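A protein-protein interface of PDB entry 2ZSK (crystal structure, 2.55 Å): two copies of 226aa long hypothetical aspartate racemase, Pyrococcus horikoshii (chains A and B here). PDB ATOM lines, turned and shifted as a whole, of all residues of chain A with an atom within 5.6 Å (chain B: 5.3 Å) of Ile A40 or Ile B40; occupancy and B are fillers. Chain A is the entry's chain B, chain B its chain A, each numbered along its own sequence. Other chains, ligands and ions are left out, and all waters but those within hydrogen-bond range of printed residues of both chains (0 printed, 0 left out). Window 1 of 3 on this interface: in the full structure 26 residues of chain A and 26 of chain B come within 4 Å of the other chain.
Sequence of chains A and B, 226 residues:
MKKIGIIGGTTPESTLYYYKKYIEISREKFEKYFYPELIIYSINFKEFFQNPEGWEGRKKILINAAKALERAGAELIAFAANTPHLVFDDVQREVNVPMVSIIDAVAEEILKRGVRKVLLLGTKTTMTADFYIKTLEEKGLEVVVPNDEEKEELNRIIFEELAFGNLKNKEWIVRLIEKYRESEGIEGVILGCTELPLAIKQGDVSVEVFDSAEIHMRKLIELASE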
ATOM      1  N   ILE A   4      -2.971  17.248  20.972  1.00  0.00           N
ATOM      2  CA  ILE A   4      -3.877  16.288  21.595  1.00  0.00           C
ATOM      3  C   ILE A   4      -5.352  16.694  21.507  1.00  0.00           C
ATOM      4  O   ILE A   4      -5.724  17.837  21.775  1.00  0.00           O
ATOM      5  CB  ILE A   4      -3.517  16.075  23.085  1.00  0.00           C
ATOM      6  CG1 ILE A   4      -2.145  15.420  23.206  1.00  0.00           C
ATOM      7  CG2 ILE A   4      -4.556  15.199  23.758  1.00  0.00           C
ATOM      8  CD1 ILE A   4      -1.611  15.414  24.630  1.00  0.00           C
ATOM      9  N   ILE A   6      -9.288  15.685  22.719  1.00  0.00           N
ATOM     10  CA  ILE A   6     -10.080  14.959  23.692  1.00  0.00           C
ATOM     11  C   ILE A   6     -11.575  15.202  23.520  1.00  0.00           C
ATOM     12  O   ILE A   6     -12.058  16.339  23.555  1.00  0.00           O
ATOM     13  CB  ILE A   6      -9.600  15.293  25.155  1.00  0.00           C
ATOM     14  CG1 ILE A   6      -8.373  14.430  25.480  1.00  0.00           C
ATOM     15  CG2 ILE A   6     -10.690  15.007  26.186  1.00  0.00           C
ATOM     16  CD1 ILE A   6      -7.711  14.736  26.798  1.00  0.00           C
ATOM     17  N   GLY A   8     -14.859  15.184  25.029  1.00  0.00           N
ATOM     18  CA  GLY A   8     -15.370  15.245  26.383  1.00  0.00           C
ATOM     19  C   GLY A   8     -16.842  15.564  26.511  1.00  0.00           C
ATOM     20  O   GLY A   8     -17.607  15.387  25.565  1.00  0.00           O
ATOM     21  N   THR A  15     -14.403  15.051  32.410  1.00  0.00           N
ATOM     22  CA  THR A  15     -13.508  15.827  31.569  1.00  0.00           C
ATOM     23  C   THR A  15     -12.642  16.734  32.437  1.00  0.00           C
ATOM     24  O   THR A  15     -11.472  16.995  32.122  1.00  0.00           O
ATOM     25  CB  THR A  15     -14.320  16.663  30.548  1.00  0.00           C
ATOM     26  OG1 THR A  15     -14.933  15.783  29.594  1.00  0.00           O
ATOM     27  CG2 THR A  15     -13.426  17.660  29.825  1.00  0.00           C
ATOM     28  N   TYR A  19      -8.473  16.906  32.471  1.00  0.00           N
ATOM     29  CA  TYR A  19      -7.712  18.143  32.333  1.00  0.00           C
ATOM     30  C   TYR A  19      -6.915  18.455  33.596  1.00  0.00           C
ATOM     31  O   TYR A  19      -5.892  19.140  33.542  1.00  0.00           O
ATOM     32  CB  TYR A  19      -8.630  19.313  32.002  1.00  0.00           C
ATOM     33  CG  TYR A  19      -7.877  20.561  31.602  1.00  0.00           C
ATOM     34  CD1 TYR A  19      -7.611  21.570  32.536  1.00  0.00           C
ATOM     35  CD2 TYR A  19      -7.432  20.743  30.286  1.00  0.00           C
ATOM     36  CE1 TYR A  19      -6.933  22.726  32.170  1.00  0.00           C
ATOM     37  CE2 TYR A  19      -6.749  21.896  29.914  1.00  0.00           C
ATOM     38  CZ  TYR A  19      -6.507  22.883  30.855  1.00  0.00           C
ATOM     39  OH  TYR A  19      -5.863  24.043  30.485  1.00  0.00           O
ATOM     40  N   LEU A  38      -3.447  20.988  23.794  1.00  0.00           N
ATOM     41  CA  LEU A  38      -4.568  20.097  23.996  1.00  0.00           C
ATOM     42  C   LEU A  38      -5.851  20.800  23.578  1.00  0.00           C
ATOM     43  O   LEU A  38      -6.116  21.929  23.994  1.00  0.00           O
ATOM     44  CB  LEU A  38      -4.651  19.732  25.481  1.00  0.00           C
ATOM     45  CG  LEU A  38      -5.387  18.463  25.898  1.00  0.00           C
ATOM     46  CD1 LEU A  38      -5.549  18.488  27.402  1.00  0.00           C
ATOM     47  CD2 LEU A  38      -6.750  18.366  25.219  1.00  0.00           C
ATOM     48  N   ILE A  39      -6.642  20.120  22.759  1.00  0.00           N
ATOM     49  CA  ILE A  39      -7.913  20.650  22.302  1.00  0.00           C
ATOM     50  C   ILE A  39      -8.992  19.783  22.962  1.00  0.00           C
ATOM     51  O   ILE A  39      -8.893  18.562  22.939  1.00  0.00           O
ATOM     52  CB  ILE A  39      -8.028  20.534  20.774  1.00  0.00           C
ATOM     53  CG1 ILE A  39      -6.819  21.190  20.110  1.00  0.00           C
ATOM     54  CG2 ILE A  39      -9.313  21.193  20.290  1.00  0.00           C
ATOM     55  CD1 ILE A  39      -6.624  20.781  18.636  1.00  0.00           C
ATOM     56  N   ILE A  40     -10.005  20.409  23.564  1.00  0.00           N
ATOM     57  CA  ILE A  40     -11.089  19.670  24.223  1.00  0.00           C
ATOM     58  C   ILE A  40     -12.463  20.000  23.641  1.00  0.00           C
ATOM     59  O   ILE A  40     -12.893  21.159  23.671  1.00  0.00           O
ATOM     60  CB  ILE A  40     -11.197  19.993  25.736  1.00  0.00           C
ATOM     61  CG1 ILE A  40      -9.876  19.742  26.456  1.00  0.00           C
ATOM     62  CG2 ILE A  40     -12.272  19.141  26.360  1.00  0.00           C
ATOM     63  CD1 ILE A  40      -9.935  20.111  27.935  1.00  0.00           C
ATOM     64  N   TYR A  41     -13.153  18.989  23.119  1.00  0.00           N
ATOM     65  CA  TYR A  41     -14.502  19.197  22.595  1.00  0.00           C
ATOM     66  C   TYR A  41     -15.489  18.661  23.639  1.00  0.00           C
ATOM     67  O   TYR A  41     -15.590  17.448  23.848  1.00  0.00           O
ATOM     68  CB  TYR A  41     -14.711  18.452  21.275  1.00  0.00           C
ATOM     69  CG  TYR A  41     -15.980  18.877  20.564  1.00  0.00           C
ATOM     70  CD1 TYR A  41     -15.930  19.679  19.417  1.00  0.00           C
ATOM     71  CD2 TYR A  41     -17.233  18.554  21.088  1.00  0.00           C
ATOM     72  CE1 TYR A  41     -17.098  20.157  18.820  1.00  0.00           C
ATOM     73  CE2 TYR A  41     -18.401  19.025  20.500  1.00  0.00           C
ATOM     74  CZ  TYR A  41     -18.327  19.827  19.371  1.00  0.00           C
ATOM     75  OH  TYR A  41     -19.479  20.325  18.824  1.00  0.00           O
ATOM     76  N   SER A  42     -16.218  19.561  24.291  1.00  0.00           N
ATOM     77  CA  SER A  42     -17.169  19.149  25.320  1.00  0.00           C
ATOM     78  C   SER A  42     -18.576  19.143  24.743  1.00  0.00           C
ATOM     79  O   SER A  42     -19.170  20.198  24.513  1.00  0.00           O
ATOM     80  CB  SER A  42     -17.087  20.096  26.525  1.00  0.00           C
ATOM     81  OG  SER A  42     -17.458  19.445  27.719  1.00  0.00           O
ATOM     82  N   LEU A  69     -12.332  18.171  16.237  1.00  0.00           N
ATOM     83  CA  LEU A  69     -10.971  18.230  16.777  1.00  0.00           C
ATOM     84  C   LEU A  69      -9.953  18.109  15.643  1.00  0.00           C
ATOM     85  O   LEU A  69      -8.943  18.818  15.630  1.00  0.00           O
ATOM     86  CB  LEU A  69     -10.767  17.107  17.797  1.00  0.00           C
ATOM     87  CG  LEU A  69     -11.696  17.156  19.026  1.00  0.00           C
ATOM     88  CD1 LEU A  69     -11.424  15.967  19.937  1.00  0.00           C
ATOM     89  CD2 LEU A  69     -11.473  18.456  19.784  1.00  0.00           C
ATOM     90  N   ILE B   6     -13.165  28.648  23.677  1.00  0.00           N
ATOM     91  CA  ILE B   6     -12.337  29.258  24.711  1.00  0.00           C
ATOM     92  C   ILE B   6     -10.863  28.992  24.460  1.00  0.00           C
ATOM     93  O   ILE B   6     -10.448  27.857  24.233  1.00  0.00           O
ATOM     94  CB  ILE B   6     -12.722  28.709  26.137  1.00  0.00           C
ATOM     95  CG1 ILE B   6     -13.984  29.397  26.640  1.00  0.00           C
ATOM     96  CG2 ILE B   6     -11.588  28.913  27.133  1.00  0.00           C
ATOM     97  CD1 ILE B   6     -14.322  29.039  28.063  1.00  0.00           C
ATOM     98  N   GLY B   8      -7.516  28.793  26.068  1.00  0.00           N
ATOM     99  CA  GLY B   8      -6.934  28.641  27.386  1.00  0.00           C
ATOM    100  C   GLY B   8      -5.461  28.344  27.308  1.00  0.00           C
ATOM    101  O   GLY B   8      -4.789  28.755  26.362  1.00  0.00           O
ATOM    102  N   THR B  15      -7.955  27.897  33.146  1.00  0.00           N
ATOM    103  CA  THR B  15      -8.875  27.223  32.229  1.00  0.00           C
ATOM    104  C   THR B  15      -9.669  26.190  33.026  1.00  0.00           C
ATOM    105  O   THR B  15     -10.864  26.023  32.812  1.00  0.00           O
ATOM    106  CB  THR B  15      -8.118  26.488  31.068  1.00  0.00           C
ATOM    107  OG1 THR B  15      -7.430  27.442  30.244  1.00  0.00           O
ATOM    108  CG2 THR B  15      -9.096  25.696  30.209  1.00  0.00           C
ATOM    109  N   TYR B  19     -13.889  25.864  33.341  1.00  0.00           N
ATOM    110  CA  TYR B  19     -14.682  24.675  33.072  1.00  0.00           C
ATOM    111  C   TYR B  19     -15.584  24.317  34.248  1.00  0.00           C
ATOM    112  O   TYR B  19     -16.736  23.913  34.065  1.00  0.00           O
ATOM    113  CB  TYR B  19     -13.775  23.495  32.732  1.00  0.00           C
ATOM    114  CG  TYR B  19     -14.503  22.382  32.006  1.00  0.00           C
ATOM    115  CD1 TYR B  19     -14.731  21.161  32.622  1.00  0.00           C
ATOM    116  CD2 TYR B  19     -14.958  22.555  30.699  1.00  0.00           C
ATOM    117  CE1 TYR B  19     -15.384  20.131  31.958  1.00  0.00           C
ATOM    118  CE2 TYR B  19     -15.619  21.530  30.016  1.00  0.00           C
ATOM    119  CZ  TYR B  19     -15.826  20.319  30.654  1.00  0.00           C
ATOM    120  OH  TYR B  19     -16.461  19.289  30.005  1.00  0.00           O
ATOM    121  N   LEU B  38     -19.126  23.277  24.173  1.00  0.00           N
ATOM    122  CA  LEU B  38     -18.001  24.148  24.479  1.00  0.00           C
ATOM    123  C   LEU B  38     -16.697  23.539  23.992  1.00  0.00           C
ATOM    124  O   LEU B  38     -16.401  22.376  24.258  1.00  0.00           O
ATOM    125  CB  LEU B  38     -17.955  24.402  25.996  1.00  0.00           C
ATOM    126  CG  LEU B  38     -16.925  25.285  26.713  1.00  0.00           C
ATOM    127  CD1 LEU B  38     -15.799  24.423  27.212  1.00  0.00           C
ATOM    128  CD2 LEU B  38     -16.413  26.394  25.802  1.00  0.00           C
ATOM    129  N   ILE B  39     -15.925  24.323  23.250  1.00  0.00           N
ATOM    130  CA  ILE B  39     -14.641  23.856  22.744  1.00  0.00           C
ATOM    131  C   ILE B  39     -13.537  24.678  23.401  1.00  0.00           C
ATOM    132  O   ILE B  39     -13.677  25.891  23.601  1.00  0.00           O
ATOM    133  CB  ILE B  39     -14.519  24.021  21.225  1.00  0.00           C
ATOM    134  CG1 ILE B  39     -15.806  23.555  20.534  1.00  0.00           C
ATOM    135  CG2 ILE B  39     -13.342  23.201  20.726  1.00  0.00           C
ATOM    136  CD1 ILE B  39     -15.840  23.886  19.035  1.00  0.00           C
ATOM    137  N   ILE B  40     -12.431  24.013  23.711  1.00  0.00           N
ATOM    138  CA  ILE B  40     -11.305  24.661  24.362  1.00  0.00           C
ATOM    139  C   ILE B  40      -9.985  24.369  23.681  1.00  0.00           C
ATOM    140  O   ILE B  40      -9.704  23.227  23.328  1.00  0.00           O
ATOM    141  CB  ILE B  40     -11.155  24.189  25.816  1.00  0.00           C
ATOM    142  CG1 ILE B  40     -12.470  24.398  26.569  1.00  0.00           C
ATOM    143  CG2 ILE B  40     -10.000  24.927  26.476  1.00  0.00           C
ATOM    144  CD1 ILE B  40     -12.464  23.829  27.943  1.00  0.00           C
ATOM    145  N   TYR B  41      -9.180  25.409  23.500  1.00  0.00           N
ATOM    146  CA  TYR B  41      -7.860  25.253  22.912  1.00  0.00           C
ATOM    147  C   TYR B  41      -6.896  25.680  24.001  1.00  0.00           C
ATOM    148  O   TYR B  41      -6.778  26.872  24.314  1.00  0.00           O
ATOM    149  CB  TYR B  41      -7.654  26.144  21.689  1.00  0.00           C
ATOM    150  CG  TYR B  41      -6.479  25.701  20.860  1.00  0.00           C
ATOM    151  CD1 TYR B  41      -6.662  24.861  19.764  1.00  0.00           C
ATOM    152  CD2 TYR B  41      -5.172  26.051  21.217  1.00  0.00           C
ATOM    153  CE1 TYR B  41      -5.575  24.371  19.043  1.00  0.00           C
ATOM    154  CE2 TYR B  41      -4.075  25.565  20.507  1.00  0.00           C
ATOM    155  CZ  TYR B  41      -4.286  24.720  19.421  1.00  0.00           C
ATOM    156  OH  TYR B  41      -3.220  24.196  18.722  1.00  0.00           O
ATOM    157  N   SER B  42      -6.223  24.704  24.591  1.00  0.00           N
ATOM    158  CA  SER B  42      -5.284  24.988  25.658  1.00  0.00           C
ATOM    159  C   SER B  42      -3.893  25.056  25.044  1.00  0.00           C
ATOM    160  O   SER B  42      -3.337  24.039  24.640  1.00  0.00           O
ATOM    161  CB  SER B  42      -5.373  23.892  26.728  1.00  0.00           C
ATOM    162  OG  SER B  42      -4.915  24.373  27.976  1.00  0.00           O
ATOM    163  N   LEU B  69     -10.255  27.126  16.807  1.00  0.00           N
ATOM    164  CA  LEU B  69     -11.584  27.016  17.399  1.00  0.00           C
ATOM    165  C   LEU B  69     -12.672  27.257  16.332  1.00  0.00           C
ATOM    166  O   LEU B  69     -13.668  26.520  16.280  1.00  0.00           O
ATOM    167  CB  LEU B  69     -11.724  27.987  18.590  1.00  0.00           C
ATOM    168  CG  LEU B  69     -10.903  27.645  19.876  1.00  0.00           C
ATOM    169  CD1 LEU B  69     -10.874  28.822  20.816  1.00  0.00           C
ATOM    170  CD2 LEU B  69     -11.494  26.437  20.581  1.00  0.00           C
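The backbone NH (N) of Tyr B41 sits at hydrogen-bond distance from the backbone carbonyl oxygen (O) of Ile B6, 2.9 Å away.
O of Tyr B41 lies within hydrogen-bond range of N of Gly B8, at 2.7 Å.
The backbone carbonyl oxygen (O) of Ile A4 is in hydrogen-bond range of the backbone NH (N) of Ile A39, at 2.7 Å.
N of Ile A6 sits at hydrogen-bond distance from O of Ile A39 (2.9 Å).
O of Ile A6 is in hydrogen-bond range of N of Tyr A41 (2.9 Å).
The backbone carbonyl oxygen (O) of Tyr A41 sits at hydrogen-bond distance from the backbone NH (N) of Gly A8, at 2.7 Å.
OH of Tyr B19 lies within hydrogen-bond range of OG of Ser A42.
The backbone NH of Ser A42 sits at hydrogen-bond distance from the backbone carbonyl oxygen of Leu B38.
The backbone carbonyl oxygen (O) of Ile B40 is in hydrogen-bond range of the backbone NH (N) of Ile A40 (2.8 Å).
The side-chain hydroxyl (OH) of Tyr A19 sits at hydrogen-bond distance from the side-chain hydroxyl (OG) of Ser B42, at 2.7 Å.
The backbone NH (N) of Ser B42 sits at hydrogen-bond distance from the backbone carbonyl oxygen (O) of Leu A38 (2.8 Å).
Thr A15 touches Tyr B19, and with the chains exchanged Tyr A19 touches Thr B15.
Tyr A19 touches Ser B42, and with the chains exchanged Ser A42 touches Tyr B19.
Leu A38 touches Ile B40, and with the chains exchanged Ile A40 touches Leu B38.
Leu A38 touches Ser B42, and with the chains exchanged Ser A42 touches Leu B38.
Positions printed for both chains: 6, 8, 15, 19, 38, 39, 40, 41, 42 and 69.
Of the 11 printed residues of chain A, 7 touch a printed residue of chain B.
Printed residues of chain A that touch a printed residue of chain B: Thr A15, Tyr A19, Leu A38, Ile A39, Ile A40, Tyr A41 and Ser A42.
Hydrophobic or aromatic side chains of chain B that line the printed part of chain A: Tyr B19, Ile B39 and Tyr B41.
Printed residues of chain B within 4 Å of Ile A39: Ile B40 (3.3 Å) and Tyr B41 (3.6 Å).
Ile A40 touches just these residues of chain B: Leu B38, Ile B39 and Ile B40.
Ile B6 touches none of the printed residues of chain A.
Of the printed residues of chain A, Ser B42 touches Tyr A19 (2.7 Å) and Leu A38 (2.8 Å).
Tyr B19 touches Thr A15 (OH to CB, 3.4 Å).
Tyr A19 touches Thr B15 (OH to CB, 3.4 Å).
Ile B40 touches Leu A38 (O to O, 3.9 Å).
C of Tyr B41 touches O of Leu A38, 3.8 Å away.
Ile B40 touches Ile A39 (O to CA, 3.3 Å).
Ile A39 touches Tyr B41 (CG1 to CE1, 3.6 Å).
Ile A40 touches Leu B38 (O to O, 3.8 Å).
Ile A40 touches Ile B39.
Tyr A41 touches Leu B38.
Tyr A41 touches Ile B39.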
